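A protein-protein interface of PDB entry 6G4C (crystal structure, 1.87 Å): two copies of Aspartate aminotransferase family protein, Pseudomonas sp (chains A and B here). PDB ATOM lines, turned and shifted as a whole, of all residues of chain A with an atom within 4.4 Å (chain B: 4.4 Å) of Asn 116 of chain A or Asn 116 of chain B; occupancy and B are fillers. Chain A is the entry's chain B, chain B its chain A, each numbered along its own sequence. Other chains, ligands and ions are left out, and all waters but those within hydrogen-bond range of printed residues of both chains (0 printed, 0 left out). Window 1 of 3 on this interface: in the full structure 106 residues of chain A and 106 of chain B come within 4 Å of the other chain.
Among the printed residues, merely in contact across the chains: Asn 116 of chain A with Pro 295 of chain B, Pro 295 of chain A with Asn 116 of chain B, Ser 117 of chain A with Asn 116 of chain B, Asn 116 of chain A with Asn 116 of chain B, Asn 116 of chain A with Ser 117 of chain B, Phe 323 of chain A with Ser 117 of chain B and Ser 117 of chain A with Phe 323 of chain B.
Asn 116 of chain A touches three residues of chain B. Printed residues of chain B within 4 Å of Ser 117 of chain A: Asn 116 (3.6 Å), Glu 120 (2.5 Å) and Phe 323 (3.96 Å). Of the printed residues of chain B, Glu 120 of chain A touches Ser 117 (2.6 Å) and Glu 120 (3.3 Å). Of the printed residues of chain B, Pro 295 of chain A touches Asn 116. Of chain A, only Asn 116, Ser 117 and Pro 295 come within 4 Å of Asn 116 of chain B. Printed residues of chain A within 4 Å of Ser 117 of chain B: Asn 116 (3.6 Å), Glu 120 (2.6 Å) and Phe 323 (3.96 Å). Of the printed residues of chain A, Glu 120 of chain B touches Ser 117 (2.5 Å) and Glu 120 (3.3 Å).
The backbone NH (N) of Asn 116 of chain A lies within hydrogen-bond range of the side-chain carboxylate (OE1) of Glu 120 of chain A (2.6 Å). The side-chain hydroxyl (OG1) of Thr 115 of chain A sits at hydrogen-bond distance from the backbone carbonyl oxygen (O) of Ser 117 of chain A (3.0 Å). The backbone carbonyl oxygen (O) of Ser 117 of chain B sits at hydrogen-bond distance from the side-chain hydroxyl (OG1) of Thr 115 of chain B (2.9 Å). The side-chain hydroxyl (OG) of Ser 117 of chain B sits at hydrogen-bond distance from the backbone NH (N) of Glu 120 of chain B, 2.9 Å away. The backbone NH (N) of Asn 116 of chain B sits at hydrogen-bond distance from the side-chain carboxylate (OE1) of Glu 120 of chain B, at 2.6 Å. The backbone carbonyl oxygen of Asn 116 of chain B lies within hydrogen-bond range of the backbone NH of Ile 296 of chain B, at 3.0 Å.
Asn 116 of chain B touches its own counterpart, Asn 116 of chain A. Asn 116 of chain A touches Ser 117 of chain B, and with the chains exchanged Ser 117 of chain A touches Asn 116 of chain B. Ser 117 of chain A touches Glu 120 of chain B, and with the chains exchanged Glu 120 of chain A touches Ser 117 of chain B. Ser 117 of chain A touches Phe 323 of chain B, and with the chains exchanged Phe 323 of chain A touches Ser 117 of chain B. Of the 10 pairs that touch across the chains among the printed residues, 10 have their exchanged pair printed and touching as well.
The side-chain hydroxyl of Ser 117 of chain B sits at hydrogen-bond distance from the side-chain carboxylate of Glu 120 of chain A, at 2.6 Å. OE2 of Glu 120 of chain B sits close to OE2 of Glu 120 of chain A (3.3 Å). The side-chain hydroxyl (OG) of Ser 117 of chain A is in hydrogen-bond range of the side-chain carboxylate (OE2) of Glu 120 of chain B.
Of the 9 printed residues of chain A, 5 touch a printed residue of chain B. Hydrophobic or aromatic side chains of chain A that line the printed part of chain B: Pro 295 and Phe 323. Hydrophobic or aromatic side chains of chain B within 4 Å of the printed part of chain A: Pro 295 and Phe 323. Among the printed residues, no Asp or Glu carboxylate lies within 4 Å of a Lys or Arg side-chain nitrogen of the other chain.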
ATOM      1  N   THR A 115       5.894 -10.295  13.884  1.00  0.00           N
ATOM      2  CA  THR A 115       5.672  -9.023  13.216  1.00  0.00           C
ATOM      3  C   THR A 115       4.724  -8.187  14.062  1.00  0.00           C
ATOM      4  O   THR A 115       4.286  -8.611  15.140  1.00  0.00           O
ATOM      5  CB  THR A 115       5.082  -9.198  11.805  1.00  0.00           C
ATOM      6  OG1 THR A 115       3.728  -9.691  11.898  1.00  0.00           O
ATOM      7  CG2 THR A 115       5.922 -10.156  10.945  1.00  0.00           C
ATOM      8  N   ASN A 116       4.371  -7.004  13.571  1.00  0.00           N
ATOM      9  CA  ASN A 116       3.370  -6.184  14.253  1.00  0.00           C
ATOM     10  C   ASN A 116       1.925  -6.545  13.864  1.00  0.00           C
ATOM     11  O   ASN A 116       1.038  -6.537  14.716  1.00  0.00           O
ATOM     12  CB  ASN A 116       3.604  -4.685  13.983  1.00  0.00           C
ATOM     13  CG  ASN A 116       5.022  -4.244  14.264  1.00  0.00           C
ATOM     14  OD1 ASN A 116       5.463  -4.202  15.404  1.00  0.00           O
ATOM     15  ND2 ASN A 116       5.763  -3.928  13.203  1.00  0.00           N
ATOM     16  N   SER A 117       1.672  -6.754  12.581  1.00  0.00           N
ATOM     17  CA  SER A 117       0.295  -6.929  12.075  1.00  0.00           C
ATOM     18  C   SER A 117       0.115  -8.237  11.336  1.00  0.00           C
ATOM     19  O   SER A 117       1.094  -8.842  10.867  1.00  0.00           O
ATOM     20  CB  SER A 117      -0.091  -5.801  11.124  1.00  0.00           C
ATOM     21  OG  SER A 117       0.730  -5.810   9.947  1.00  0.00           O
ATOM     22  N   GLU A 120       1.412  -7.607   7.767  1.00  0.00           N
ATOM     23  CA  GLU A 120       2.856  -7.816   7.714  1.00  0.00           C
ATOM     24  C   GLU A 120       3.236  -9.288   7.795  1.00  0.00           C
ATOM     25  O   GLU A 120       4.179  -9.715   7.140  1.00  0.00           O
ATOM     26  CB  GLU A 120       3.560  -7.160   8.877  1.00  0.00           C
ATOM     27  CG  GLU A 120       3.750  -5.669   8.848  1.00  0.00           C
ATOM     28  CD  GLU A 120       4.253  -5.198  10.192  1.00  0.00           C
ATOM     29  OE1 GLU A 120       4.128  -5.981  11.164  1.00  0.00           O
ATOM     30  OE2 GLU A 120       4.750  -4.053  10.297  1.00  0.00           O
ATOM     31  N   PRO A 295      -0.078  -4.254  19.386  1.00  0.00           N
ATOM     32  CA  PRO A 295       0.051  -4.765  18.006  1.00  0.00           C
ATOM     33  C   PRO A 295       1.105  -5.845  17.941  1.00  0.00           C
ATOM     34  O   PRO A 295       2.286  -5.579  18.137  1.00  0.00           O
ATOM     35  CB  PRO A 295       0.475  -3.546  17.184  1.00  0.00           C
ATOM     36  CG  PRO A 295       0.366  -2.376  18.085  1.00  0.00           C
ATOM     37  CD  PRO A 295       0.451  -2.882  19.512  1.00  0.00           C
ATOM     38  N   ILE A 296       0.683  -7.065  17.673  1.00  0.00           N
ATOM     39  CA  ILE A 296       1.635  -8.157  17.501  1.00  0.00           C
ATOM     40  C   ILE A 296       0.983  -9.226  16.644  1.00  0.00           C
ATOM     41  O   ILE A 296      -0.221  -9.518  16.753  1.00  0.00           O
ATOM     42  CB  ILE A 296       2.139  -8.742  18.852  1.00  0.00           C
ATOM     43  CG1 ILE A 296       3.034  -9.975  18.639  1.00  0.00           C
ATOM     44  CG2 ILE A 296       0.980  -9.104  19.774  1.00  0.00           C
ATOM     45  CD1 ILE A 296       3.784 -10.404  19.879  1.00  0.00           C
ATOM     46  N   ALA A 297       1.790  -9.820  15.780  1.00  0.00           N
ATOM     47  CA  ALA A 297       1.383 -11.017  15.066  1.00  0.00           C
ATOM     48  C   ALA A 297       2.556 -12.009  15.103  1.00  0.00           C
ATOM     49  O   ALA A 297       3.706 -11.627  15.348  1.00  0.00           O
ATOM     50  CB  ALA A 297       1.023 -10.666  13.655  1.00  0.00           C
ATOM     51  N   PHE A 323      11.220  -6.428  11.166  1.00  0.00           N
ATOM     52  CA  PHE A 323      10.641  -5.123  11.478  1.00  0.00           C
ATOM     53  C   PHE A 323      11.254  -4.632  12.779  1.00  0.00           C
ATOM     54  O   PHE A 323      11.598  -5.429  13.654  1.00  0.00           O
ATOM     55  CB  PHE A 323       9.137  -5.224  11.663  1.00  0.00           C
ATOM     56  CG  PHE A 323       8.427  -5.734  10.450  1.00  0.00           C
ATOM     57  CD1 PHE A 323       8.236  -7.102  10.269  1.00  0.00           C
ATOM     58  CD2 PHE A 323       7.987  -4.860   9.479  1.00  0.00           C
ATOM     59  CE1 PHE A 323       7.604  -7.584   9.142  1.00  0.00           C
ATOM     60  CE2 PHE A 323       7.376  -5.353   8.324  1.00  0.00           C
ATOM     61  CZ  PHE A 323       7.185  -6.704   8.163  1.00  0.00           C
ATOM     62  N   GLY A 325       9.758  -3.498  15.238  1.00  0.00           N
ATOM     63  CA  GLY A 325       8.890  -3.997  16.310  1.00  0.00           C
ATOM     64  C   GLY A 325       8.744  -5.509  16.400  1.00  0.00           C
ATOM     65  O   GLY A 325       7.981  -5.997  17.243  1.00  0.00           O
ATOM     66  N   THR B 115      -0.010   3.655  10.848  1.00  0.00           N
ATOM     67  CA  THR B 115       0.273   2.232  10.709  1.00  0.00           C
ATOM     68  C   THR B 115       1.095   1.778  11.915  1.00  0.00           C
ATOM     69  O   THR B 115       1.354   2.566  12.830  1.00  0.00           O
ATOM     70  CB  THR B 115       1.053   1.929   9.412  1.00  0.00           C
ATOM     71  OG1 THR B 115       2.370   2.470   9.509  1.00  0.00           O
ATOM     72  CG2 THR B 115       0.347   2.513   8.170  1.00  0.00           C
ATOM     73  N   ASN B 116       1.508   0.514  11.929  1.00  0.00           N
ATOM     74  CA  ASN B 116       2.372   0.013  13.001  1.00  0.00           C
ATOM     75  C   ASN B 116       3.845   0.232  12.716  1.00  0.00           C
ATOM     76  O   ASN B 116       4.590   0.574  13.618  1.00  0.00           O
ATOM     77  CB  ASN B 116       2.155  -1.476  13.244  1.00  0.00           C
ATOM     78  CG  ASN B 116       0.697  -1.817  13.473  1.00  0.00           C
ATOM     79  OD1 ASN B 116       0.100  -1.451  14.505  1.00  0.00           O
ATOM     80  ND2 ASN B 116       0.110  -2.492  12.516  1.00  0.00           N
ATOM     81  N   SER B 117       4.271   0.015  11.475  1.00  0.00           N
ATOM     82  CA  SER B 117       5.692   0.064  11.120  1.00  0.00           C
ATOM     83  C   SER B 117       5.986   1.035   9.996  1.00  0.00           C
ATOM     84  O   SER B 117       5.094   1.410   9.220  1.00  0.00           O
ATOM     85  CB  SER B 117       6.193  -1.319  10.694  1.00  0.00           C
ATOM     86  OG  SER B 117       5.537  -1.754   9.516  1.00  0.00           O
ATOM     87  N   GLU B 120       5.197  -0.857   6.767  1.00  0.00           N
ATOM     88  CA  GLU B 120       3.776  -0.720   6.419  1.00  0.00           C
ATOM     89  C   GLU B 120       3.423   0.670   5.903  1.00  0.00           C
ATOM     90  O   GLU B 120       2.598   0.803   5.012  1.00  0.00           O
ATOM     91  CB  GLU B 120       2.888  -0.966   7.621  1.00  0.00           C
ATOM     92  CG  GLU B 120       2.698  -2.370   8.104  1.00  0.00           C
ATOM     93  CD  GLU B 120       2.033  -2.364   9.482  1.00  0.00           C
ATOM     94  OE1 GLU B 120       2.003  -1.270  10.106  1.00  0.00           O
ATOM     95  OE2 GLU B 120       1.531  -3.415   9.932  1.00  0.00           O
ATOM     96  N   PRO B 295       4.959   0.150  18.908  1.00  0.00           N
ATOM     97  CA  PRO B 295       5.076   0.146  17.445  1.00  0.00           C
ATOM     98  C   PRO B 295       4.043   1.081  16.840  1.00  0.00           C
ATOM     99  O   PRO B 295       2.850   0.865  16.987  1.00  0.00           O
ATOM    100  CB  PRO B 295       4.797  -1.310  17.043  1.00  0.00           C
ATOM    101  CG  PRO B 295       4.761  -2.073  18.300  1.00  0.00           C
ATOM    102  CD  PRO B 295       4.480  -1.132  19.435  1.00  0.00           C
ATOM    103  N   ILE B 296       4.512   2.139  16.196  1.00  0.00           N
ATOM    104  CA  ILE B 296       3.613   3.066  15.527  1.00  0.00           C
ATOM    105  C   ILE B 296       4.396   3.803  14.439  1.00  0.00           C
ATOM    106  O   ILE B 296       5.579   4.094  14.598  1.00  0.00           O
ATOM    107  CB  ILE B 296       2.947   4.055  16.519  1.00  0.00           C
ATOM    108  CG1 ILE B 296       2.101   5.091  15.777  1.00  0.00           C
ATOM    109  CG2 ILE B 296       3.980   4.753  17.402  1.00  0.00           C
ATOM    110  CD1 ILE B 296       1.205   5.897  16.676  1.00  0.00           C
ATOM    111  N   ALA B 297       3.723   4.073  13.326  1.00  0.00           N
ATOM    112  CA  ALA B 297       4.267   4.915  12.310  1.00  0.00           C
ATOM    113  C   ALA B 297       3.139   5.797  11.826  1.00  0.00           C
ATOM    114  O   ALA B 297       1.960   5.491  12.048  1.00  0.00           O
ATOM    115  CB  ALA B 297       4.827   4.077  11.156  1.00  0.00           C
ATOM    116  N   PHE B 323      -4.950  -1.051   9.059  1.00  0.00           N
ATOM    117  CA  PHE B 323      -4.466  -2.133   9.879  1.00  0.00           C
ATOM    118  C   PHE B 323      -5.273  -2.174  11.158  1.00  0.00           C
ATOM    119  O   PHE B 323      -5.693  -1.149  11.648  1.00  0.00           O
ATOM    120  CB  PHE B 323      -2.987  -1.953  10.205  1.00  0.00           C
ATOM    121  CG  PHE B 323      -2.124  -1.884   8.988  1.00  0.00           C
ATOM    122  CD1 PHE B 323      -1.637  -3.033   8.410  1.00  0.00           C
ATOM    123  CD2 PHE B 323      -1.877  -0.666   8.373  1.00  0.00           C
ATOM    124  CE1 PHE B 323      -0.870  -2.970   7.261  1.00  0.00           C
ATOM    125  CE2 PHE B 323      -1.118  -0.589   7.227  1.00  0.00           C
ATOM    126  CZ  PHE B 323      -0.614  -1.744   6.666  1.00  0.00           C
ATOM    127  N   GLY B 325      -4.153  -2.333  14.046  1.00  0.00           N
ATOM    128  CA  GLY B 325      -3.457  -1.453  14.983  1.00  0.00           C
ATOM    129  C   GLY B 325      -3.290  -0.012  14.542  1.00  0.00           C
ATOM    130  O   GLY B 325      -2.640   0.776  15.251  1.00  0.00           O
